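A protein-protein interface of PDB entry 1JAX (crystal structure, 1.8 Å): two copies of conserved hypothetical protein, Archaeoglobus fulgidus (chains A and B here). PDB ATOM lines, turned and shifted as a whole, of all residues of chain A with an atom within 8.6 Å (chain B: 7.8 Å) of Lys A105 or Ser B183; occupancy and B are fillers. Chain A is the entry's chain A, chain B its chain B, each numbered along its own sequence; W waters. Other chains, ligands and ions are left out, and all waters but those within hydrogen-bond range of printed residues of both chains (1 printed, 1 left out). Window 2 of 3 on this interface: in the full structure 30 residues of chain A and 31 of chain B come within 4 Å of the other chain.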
ATOM      1  N   SER A 101      -7.889 -28.549  -6.733  1.00  0.00           N
ATOM      2  CA  SER A 101      -8.994 -28.314  -5.823  1.00  0.00           C
ATOM      3  C   SER A 101     -10.248 -28.394  -6.668  1.00  0.00           C
ATOM      4  O   SER A 101     -10.249 -27.975  -7.822  1.00  0.00           O
ATOM      5  CB  SER A 101      -8.877 -26.934  -5.178  1.00  0.00           C
ATOM      6  OG  SER A 101     -10.007 -26.670  -4.367  1.00  0.00           O
ATOM      7  N   ARG A 102     -11.323 -28.935  -6.101  1.00  0.00           N
ATOM      8  CA  ARG A 102     -12.573 -29.059  -6.828  1.00  0.00           C
ATOM      9  C   ARG A 102     -13.635 -28.197  -6.143  1.00  0.00           C
ATOM     10  O   ARG A 102     -13.933 -28.397  -4.964  1.00  0.00           O
ATOM     11  CB  ARG A 102     -13.020 -30.517  -6.817  1.00  0.00           C
ATOM     12  CG  ARG A 102     -14.345 -30.725  -7.509  1.00  0.00           C
ATOM     13  CD  ARG A 102     -14.755 -32.203  -7.494  1.00  0.00           C
ATOM     14  NE  ARG A 102     -16.077 -32.384  -8.099  1.00  0.00           N
ATOM     15  CZ  ARG A 102     -16.774 -33.507  -8.013  1.00  0.00           C
ATOM     16  NH1 ARG A 102     -16.268 -34.547  -7.346  1.00  0.00           N
ATOM     17  NH2 ARG A 102     -17.980 -33.585  -8.577  1.00  0.00           N
ATOM     18  N   GLY A 103     -14.201 -27.246  -6.874  1.00  0.00           N
ATOM     19  CA  GLY A 103     -15.192 -26.369  -6.273  1.00  0.00           C
ATOM     20  C   GLY A 103     -16.415 -26.166  -7.130  1.00  0.00           C
ATOM     21  O   GLY A 103     -16.557 -26.768  -8.204  1.00  0.00           O
ATOM     22  N   ALA A 104     -17.289 -25.284  -6.654  1.00  0.00           N
ATOM     23  CA  ALA A 104     -18.533 -24.971  -7.327  1.00  0.00           C
ATOM     24  C   ALA A 104     -18.319 -24.454  -8.750  1.00  0.00           C
ATOM     25  O   ALA A 104     -19.134 -24.719  -9.643  1.00  0.00           O
ATOM     26  CB  ALA A 104     -19.315 -23.940  -6.508  1.00  0.00           C
ATOM     27  N   LYS A 105     -17.233 -23.719  -8.956  1.00  0.00           N
ATOM     28  CA  LYS A 105     -16.949 -23.146 -10.267  1.00  0.00           C
ATOM     29  C   LYS A 105     -15.973 -23.959 -11.121  1.00  0.00           C
ATOM     30  O   LYS A 105     -15.521 -23.495 -12.168  1.00  0.00           O
ATOM     31  CB  LYS A 105     -16.440 -21.706 -10.099  1.00  0.00           C
ATOM     32  CG  LYS A 105     -17.481 -20.776  -9.466  1.00  0.00           C
ATOM     33  CD  LYS A 105     -16.975 -19.353  -9.292  1.00  0.00           C
ATOM     34  CE  LYS A 105     -16.880 -18.591 -10.612  1.00  0.00           C
ATOM     35  NZ  LYS A 105     -16.283 -17.247 -10.372  1.00  0.00           N
ATOM     36  N   GLY A 106     -15.659 -25.173 -10.688  1.00  0.00           N
ATOM     37  CA  GLY A 106     -14.765 -26.011 -11.463  1.00  0.00           C
ATOM     38  C   GLY A 106     -13.527 -26.432 -10.701  1.00  0.00           C
ATOM     39  O   GLY A 106     -13.488 -26.364  -9.471  1.00  0.00           O
ATOM     40  N   PHE A 107     -12.506 -26.835 -11.451  1.00  0.00           N
ATOM     41  CA  PHE A 107     -11.255 -27.283 -10.879  1.00  0.00           C
ATOM     42  C   PHE A 107     -10.196 -26.202 -10.983  1.00  0.00           C
ATOM     43  O   PHE A 107     -10.113 -25.478 -11.989  1.00  0.00           O
ATOM     44  CB  PHE A 107     -10.793 -28.553 -11.592  1.00  0.00           C
ATOM     45  CG  PHE A 107     -11.763 -29.693 -11.465  1.00  0.00           C
ATOM     46  CD1 PHE A 107     -12.888 -29.759 -12.286  1.00  0.00           C
ATOM     47  CD2 PHE A 107     -11.563 -30.681 -10.517  1.00  0.00           C
ATOM     48  CE1 PHE A 107     -13.806 -30.814 -12.160  1.00  0.00           C
ATOM     49  CE2 PHE A 107     -12.474 -31.740 -10.374  1.00  0.00           C
ATOM     50  CZ  PHE A 107     -13.594 -31.804 -11.199  1.00  0.00           C
ATOM     51  N   THR A 108      -9.390 -26.088  -9.925  1.00  0.00           N
ATOM     52  CA  THR A 108      -8.351 -25.076  -9.888  1.00  0.00           C
ATOM     53  C   THR A 108      -7.016 -25.664  -9.434  1.00  0.00           C
ATOM     54  O   THR A 108      -6.955 -26.706  -8.787  1.00  0.00           O
ATOM     55  CB  THR A 108      -8.726 -23.916  -8.944  1.00  0.00           C
ATOM     56  OG1 THR A 108      -9.019 -24.430  -7.641  1.00  0.00           O
ATOM     57  CG2 THR A 108      -9.960 -23.205  -9.457  1.00  0.00           C
ATOM     58  N   TYR A 109      -5.951 -24.983  -9.822  1.00  0.00           N
ATOM     59  CA  TYR A 109      -4.604 -25.369  -9.450  1.00  0.00           C
ATOM     60  C   TYR A 109      -4.484 -24.825  -8.028  1.00  0.00           C
ATOM     61  O   TYR A 109      -4.542 -23.609  -7.801  1.00  0.00           O
ATOM     62  CB  TYR A 109      -3.625 -24.689 -10.378  1.00  0.00           C
ATOM     63  CG  TYR A 109      -2.244 -25.248 -10.235  1.00  0.00           C
ATOM     64  CD1 TYR A 109      -1.925 -26.489 -10.782  1.00  0.00           C
ATOM     65  CD2 TYR A 109      -1.280 -24.568  -9.515  1.00  0.00           C
ATOM     66  CE1 TYR A 109      -0.663 -27.043 -10.607  1.00  0.00           C
ATOM     67  CE2 TYR A 109      -0.015 -25.103  -9.336  1.00  0.00           C
ATOM     68  CZ  TYR A 109       0.282 -26.339  -9.892  1.00  0.00           C
ATOM     69  OH  TYR A 109       1.549 -26.848  -9.770  1.00  0.00           O
ATOM     70  N   PRO A 193      -6.127 -29.758 -14.120  1.00  0.00           N
ATOM     71  CA  PRO A 193      -7.407 -29.117 -13.789  1.00  0.00           C
ATOM     72  C   PRO A 193      -8.084 -28.544 -15.041  1.00  0.00           C
ATOM     73  O   PRO A 193      -9.309 -28.420 -15.093  1.00  0.00           O
ATOM     74  CB  PRO A 193      -7.018 -28.032 -12.763  1.00  0.00           C
ATOM     75  CG  PRO A 193      -5.523 -27.866 -12.924  1.00  0.00           C
ATOM     76  CD  PRO A 193      -5.052 -29.270 -13.240  1.00  0.00           C
ATOM     77  N   ASN A 197     -11.875 -29.524 -16.084  1.00  0.00           N
ATOM     78  CA  ASN A 197     -12.931 -28.549 -16.373  1.00  0.00           C
ATOM     79  C   ASN A 197     -13.583 -28.869 -17.710  1.00  0.00           C
ATOM     80  O   ASN A 197     -14.811 -28.843 -17.834  1.00  0.00           O
ATOM     81  CB  ASN A 197     -12.404 -27.100 -16.396  1.00  0.00           C
ATOM     82  CG  ASN A 197     -12.185 -26.548 -14.997  1.00  0.00           C
ATOM     83  OD1 ASN A 197     -13.068 -26.654 -14.143  1.00  0.00           O
ATOM     84  ND2 ASN A 197     -11.017 -25.962 -14.751  1.00  0.00           N
ATOM     85  N   ARG A 200     -15.939 -31.736 -17.271  1.00  0.00           N
ATOM     86  CA  ARG A 200     -17.160 -31.327 -16.576  1.00  0.00           C
ATOM     87  C   ARG A 200     -18.124 -30.488 -17.420  1.00  0.00           C
ATOM     88  O   ARG A 200     -19.321 -30.787 -17.506  1.00  0.00           O
ATOM     89  CB  ARG A 200     -16.818 -30.538 -15.299  1.00  0.00           C
ATOM     90  CG  ARG A 200     -18.066 -29.898 -14.651  1.00  0.00           C
ATOM     91  CD  ARG A 200     -17.795 -29.155 -13.331  1.00  0.00           C
ATOM     92  NE  ARG A 200     -19.019 -28.450 -12.920  1.00  0.00           N
ATOM     93  CZ  ARG A 200     -19.099 -27.543 -11.946  1.00  0.00           C
ATOM     94  NH1 ARG A 200     -18.032 -27.210 -11.236  1.00  0.00           N
ATOM     95  NH2 ARG A 200     -20.253 -26.930 -11.714  1.00  0.00           N
ATOM     96  N   PHE A 201     -17.606 -29.442 -18.052  1.00  0.00           N
ATOM     97  CA  PHE A 201     -18.463 -28.544 -18.809  1.00  0.00           C
ATOM     98  C   PHE A 201     -18.863 -28.941 -20.231  1.00  0.00           C
ATOM     99  O   PHE A 201     -19.691 -28.261 -20.844  1.00  0.00           O
ATOM    100  CB  PHE A 201     -17.875 -27.125 -18.753  1.00  0.00           C
ATOM    101  CG  PHE A 201     -17.780 -26.567 -17.342  1.00  0.00           C
ATOM    102  CD1 PHE A 201     -16.559 -26.515 -16.674  1.00  0.00           C
ATOM    103  CD2 PHE A 201     -18.929 -26.146 -16.665  1.00  0.00           C
ATOM    104  CE1 PHE A 201     -16.472 -26.053 -15.354  1.00  0.00           C
ATOM    105  CE2 PHE A 201     -18.857 -25.677 -15.330  1.00  0.00           C
ATOM    106  CZ  PHE A 201     -17.628 -25.632 -14.674  1.00  0.00           C
ATOM    107  N   SER B 114      -5.797 -13.548 -14.260  1.00  0.00           N
ATOM    108  CA  SER B 114      -5.783 -13.820 -15.702  1.00  0.00           C
ATOM    109  C   SER B 114      -6.040 -12.543 -16.503  1.00  0.00           C
ATOM    110  O   SER B 114      -6.596 -11.555 -15.984  1.00  0.00           O
ATOM    111  CB  SER B 114      -6.833 -14.888 -16.010  1.00  0.00           C
ATOM    112  OG  SER B 114      -8.157 -14.372 -15.936  1.00  0.00           O
ATOM    113  N   ALA B 116      -8.074 -12.271 -19.013  1.00  0.00           N
ATOM    114  CA  ALA B 116      -9.509 -12.129 -19.239  1.00  0.00           C
ATOM    115  C   ALA B 116     -10.233 -11.508 -18.053  1.00  0.00           C
ATOM    116  O   ALA B 116     -11.124 -10.664 -18.228  1.00  0.00           O
ATOM    117  CB  ALA B 116     -10.131 -13.499 -19.558  1.00  0.00           C
ATOM    118  N   GLU B 117      -9.857 -11.911 -16.845  1.00  0.00           N
ATOM    119  CA  GLU B 117     -10.544 -11.354 -15.671  1.00  0.00           C
ATOM    120  C   GLU B 117     -10.138  -9.906 -15.464  1.00  0.00           C
ATOM    121  O   GLU B 117     -10.968  -9.065 -15.083  1.00  0.00           O
ATOM    122  CB  GLU B 117     -10.240 -12.220 -14.445  1.00  0.00           C
ATOM    123  CG  GLU B 117     -10.945 -13.565 -14.501  1.00  0.00           C
ATOM    124  CD  GLU B 117     -10.416 -14.522 -13.454  1.00  0.00           C
ATOM    125  OE1 GLU B 117     -11.154 -14.846 -12.497  1.00  0.00           O
ATOM    126  OE2 GLU B 117      -9.252 -14.936 -13.586  1.00  0.00           O
ATOM    127  N   CYS B 154     -13.863 -19.862 -22.012  1.00  0.00           N
ATOM    128  CA  CYS B 154     -14.292 -19.585 -20.635  1.00  0.00           C
ATOM    129  C   CYS B 154     -15.175 -18.338 -20.613  1.00  0.00           C
ATOM    130  O   CYS B 154     -15.039 -17.446 -21.453  1.00  0.00           O
ATOM    131  CB  CYS B 154     -13.073 -19.315 -19.721  1.00  0.00           C
ATOM    132  SG  CYS B 154     -12.095 -20.764 -19.398  1.00  0.00           S
ATOM    133  N   GLY B 155     -16.050 -18.256 -19.621  1.00  0.00           N
ATOM    134  CA  GLY B 155     -16.908 -17.087 -19.548  1.00  0.00           C
ATOM    135  C   GLY B 155     -18.027 -17.291 -18.548  1.00  0.00           C
ATOM    136  O   GLY B 155     -18.496 -18.411 -18.329  1.00  0.00           O
ATOM    137  N   ASP B 156     -18.452 -16.188 -17.953  1.00  0.00           N
ATOM    138  CA  ASP B 156     -19.513 -16.217 -16.948  1.00  0.00           C
ATOM    139  C   ASP B 156     -20.932 -16.153 -17.509  1.00  0.00           C
ATOM    140  O   ASP B 156     -21.878 -16.647 -16.870  1.00  0.00           O
ATOM    141  CB  ASP B 156     -19.314 -15.058 -15.974  1.00  0.00           C
ATOM    142  CG  ASP B 156     -18.139 -15.271 -15.054  1.00  0.00           C
ATOM    143  OD1 ASP B 156     -17.635 -16.409 -14.990  1.00  0.00           O
ATOM    144  OD2 ASP B 156     -17.727 -14.297 -14.384  1.00  0.00           O
ATOM    145  N   ALA B 179     -14.836 -24.450 -21.047  1.00  0.00           N
ATOM    146  CA  ALA B 179     -13.931 -24.692 -19.923  1.00  0.00           C
ATOM    147  C   ALA B 179     -14.450 -24.081 -18.622  1.00  0.00           C
ATOM    148  O   ALA B 179     -13.726 -24.009 -17.619  1.00  0.00           O
ATOM    149  CB  ALA B 179     -12.523 -24.170 -20.247  1.00  0.00           C
ATOM    150  N   GLY B 180     -15.714 -23.648 -18.634  1.00  0.00           N
ATOM    151  CA  GLY B 180     -16.301 -23.087 -17.428  1.00  0.00           C
ATOM    152  C   GLY B 180     -16.353 -21.580 -17.288  1.00  0.00           C
ATOM    153  O   GLY B 180     -16.279 -20.843 -18.283  1.00  0.00           O
ATOM    154  N   PRO B 181     -16.485 -21.096 -16.042  1.00  0.00           N
ATOM    155  CA  PRO B 181     -16.556 -19.667 -15.703  1.00  0.00           C
ATOM    156  C   PRO B 181     -15.259 -18.942 -16.076  1.00  0.00           C
ATOM    157  O   PRO B 181     -14.235 -19.584 -16.351  1.00  0.00           O
ATOM    158  CB  PRO B 181     -16.775 -19.665 -14.181  1.00  0.00           C
ATOM    159  CG  PRO B 181     -17.356 -21.017 -13.877  1.00  0.00           C
ATOM    160  CD  PRO B 181     -16.636 -21.942 -14.843  1.00  0.00           C
ATOM    161  N   LEU B 182     -15.278 -17.614 -16.066  1.00  0.00           N
ATOM    162  CA  LEU B 182     -14.061 -16.871 -16.404  1.00  0.00           C
ATOM    163  C   LEU B 182     -12.936 -17.141 -15.405  1.00  0.00           C
ATOM    164  O   LEU B 182     -11.758 -16.863 -15.694  1.00  0.00           O
ATOM    165  CB  LEU B 182     -14.320 -15.357 -16.424  1.00  0.00           C
ATOM    166  CG  LEU B 182     -14.283 -14.490 -17.687  1.00  0.00           C
ATOM    167  CD1 LEU B 182     -13.573 -13.173 -17.319  1.00  0.00           C
ATOM    168  CD2 LEU B 182     -13.633 -15.164 -18.888  1.00  0.00           C
ATOM    169  N   SER B 183     -13.289 -17.649 -14.223  1.00  0.00           N
ATOM    170  CA  SER B 183     -12.284 -17.951 -13.203  1.00  0.00           C
ATOM    171  C   SER B 183     -11.336 -19.081 -13.614  1.00  0.00           C
ATOM    172  O   SER B 183     -10.357 -19.352 -12.911  1.00  0.00           O
ATOM    173  CB  SER B 183     -12.955 -18.289 -11.852  1.00  0.00           C
ATOM    174  OG  SER B 183     -14.020 -19.212 -12.008  1.00  0.00           O
ATOM    175  N   ASN B 184     -11.632 -19.740 -14.734  1.00  0.00           N
ATOM    176  CA  ASN B 184     -10.758 -20.805 -15.233  1.00  0.00           C
ATOM    177  C   ASN B 184      -9.891 -20.299 -16.367  1.00  0.00           C
ATOM    178  O   ASN B 184      -9.104 -21.058 -16.938  1.00  0.00           O
ATOM    179  CB  ASN B 184     -11.572 -22.004 -15.730  1.00  0.00           C
ATOM    180  CG  ASN B 184     -12.211 -22.762 -14.595  1.00  0.00           C
ATOM    181  OD1 ASN B 184     -11.693 -22.748 -13.471  1.00  0.00           O
ATOM    182  ND2 ASN B 184     -13.324 -23.437 -14.872  1.00  0.00           N
ATOM    183  N   SER B 185      -9.999 -19.008 -16.679  1.00  0.00           N
ATOM    184  CA  SER B 185      -9.234 -18.456 -17.791  1.00  0.00           C
ATOM    185  C   SER B 185      -7.723 -18.595 -17.610  1.00  0.00           C
ATOM    186  O   SER B 185      -7.007 -18.772 -18.589  1.00  0.00           O
ATOM    187  CB  SER B 185      -9.594 -16.978 -18.035  1.00  0.00           C
ATOM    188  OG  SER B 185      -9.029 -16.498 -19.252  1.00  0.00           O
ATOM    189  N   ARG B 186      -7.229 -18.515 -16.375  1.00  0.00           N
ATOM    190  CA  ARG B 186      -5.783 -18.649 -16.168  1.00  0.00           C
ATOM    191  C   ARG B 186      -5.311 -20.020 -16.679  1.00  0.00           C
ATOM    192  O   ARG B 186      -4.233 -20.139 -17.253  1.00  0.00           O
ATOM    193  CB  ARG B 186      -5.429 -18.489 -14.691  1.00  0.00           C
ATOM    194  CG  ARG B 186      -3.940 -18.367 -14.405  1.00  0.00           C
ATOM    195  CD  ARG B 186      -3.773 -17.876 -12.955  1.00  0.00           C
ATOM    196  NE  ARG B 186      -2.393 -17.585 -12.575  1.00  0.00           N
ATOM    197  CZ  ARG B 186      -1.410 -18.473 -12.625  1.00  0.00           C
ATOM    198  NH1 ARG B 186      -1.660 -19.697 -13.050  1.00  0.00           N
ATOM    199  NH2 ARG B 186      -0.193 -18.150 -12.216  1.00  0.00           N
ATOM    200  N   LEU B 187      -6.124 -21.048 -16.502  1.00  0.00           N
ATOM    201  CA  LEU B 187      -5.731 -22.400 -16.937  1.00  0.00           C
ATOM    202  C   LEU B 187      -5.687 -22.478 -18.449  1.00  0.00           C
ATOM    203  O   LEU B 187      -4.855 -23.175 -19.026  1.00  0.00           O
ATOM    204  CB  LEU B 187      -6.725 -23.444 -16.406  1.00  0.00           C
ATOM    205  CG  LEU B 187      -6.741 -23.545 -14.877  1.00  0.00           C
ATOM    206  CD1 LEU B 187      -7.875 -24.495 -14.456  1.00  0.00           C
ATOM    207  CD2 LEU B 187      -5.376 -24.054 -14.352  1.00  0.00           C
ATOM    208  N   VAL B 188      -6.599 -21.755 -19.096  1.00  0.00           N
ATOM    209  CA  VAL B 188      -6.612 -21.767 -20.554  1.00  0.00           C
ATOM    210  C   VAL B 188      -5.469 -20.907 -21.086  1.00  0.00           C
ATOM    211  O   VAL B 188      -4.755 -21.300 -22.018  1.00  0.00           O
ATOM    212  CB  VAL B 188      -7.958 -21.236 -21.106  1.00  0.00           C
ATOM    213  CG1 VAL B 188      -7.908 -21.188 -22.649  1.00  0.00           C
ATOM    214  CG2 VAL B 188      -9.107 -22.144 -20.621  1.00  0.00           C
HETATM  215  O   HOH W   1     -13.019 -21.737 -11.525  1.00  0.00           O
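Among the printed residues, merely in contact across the chains: Lys A105 with Pro B181 (3.3 Å), Phe A107 with Leu B187 (3.5 Å), Asn A197 with Leu B187 (3.5 Å), Phe A201 with Gly B180 (3.5 Å), Asn A197 with Ala B179 (3.6 Å), Phe A201 with Ala B179 (3.8 Å) and Phe A201 with Pro B181 (3.8 Å).
Water W1 lies within hydrogen-bond range of the side-chain amide oxygen of Asn B184 (2.6 Å), the side-chain hydroxyl of Ser B183 (2.8 Å) and the backbone carbonyl oxygen of Lys A105 (3.1 Å).
No position is printed for both chains.
Of the 11 pairs that touch across the chains among the printed residues, none has its exchanged pair printed and touching as well.
The backbone carbonyl oxygen of Lys A105 sits at hydrogen-bond distance from the side-chain amide nitrogen of Asn B184 (3.5 Å).
ND2 of Asn B184 lies within hydrogen-bond range of OD1 of Asn A197.
NZ of Lys A105 lies close to OG of Ser B183.
The side-chain amide oxygen of Asn B184 lies close to the backbone carbonyl oxygen of Phe A107, 3.5 Å away.
Printed residues of chain A that touch a printed residue of chain B: Lys A105, Phe A107, Asn A197 and Phe A201.
Hydrophobic or aromatic side chains of chain A that line the printed part of chain B: Phe A201.
Of the 16 printed residues of chain B, 6 touch a printed residue of chain A.
Hydrophobic or aromatic side chains of chain B that line the printed part of chain A: Pro B181 and Leu B187.
Among the printed residues, no Asp or Glu carboxylate lies within 4 Å of a Lys or Arg side-chain nitrogen of the other chain.
Gly A103 touches none of the printed residues of chain B.
Of chain B, only Pro B181, Ser B183 and Asn B184 come within 4 Å of Lys A105.
Of the printed residues of chain B, Phe A107 touches Asn B184 (3.5 Å) and Leu B187 (3.5 Å).
Tyr A109 touches none of the printed residues of chain B.
Printed residues of chain B within 4 Å of Asn A197: Ala B179 (3.6 Å), Asn B184 (3.3 Å) and Leu B187 (3.5 Å).
Printed residues of chain B within 4 Å of Phe A201: Ala B179 (3.8 Å), Gly B180 (3.5 Å) and Pro B181 (3.8 Å).
Printed residues of chain A within 4 Å of Gly B180: Phe A201 (3.5 Å).
Of chain A, only Lys A105 comes within 4 Å of Ser B183.
Of the printed residues of chain A, Leu B187 touches Phe A107 (3.5 Å) and Asn A197 (3.5 Å).
The nearest residue of chain B that does not touch Lys A105 is Asp B156 (4.9 Å).
The nearest residue of chain A that does not touch Ser B183 is Thr A108 (5.2 Å).
The nearest printed residue of chain A that does not touch Gly B180 is Asn A197 (5.3 Å).
The backbone NH (N) of Phe A107 is in hydrogen-bond range of the side-chain amide oxygen (OD1) of Asn A197 (2.8 Å).
O of Pro A193 lies within hydrogen-bond range of ND2 of Asn A197 (3.0 Å).
O of Ala B179 sits at hydrogen-bond distance from ND2 of Asn B184.
O of Gly B180 sits at hydrogen-bond distance from N of Gly B155, 2.9 Å away.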
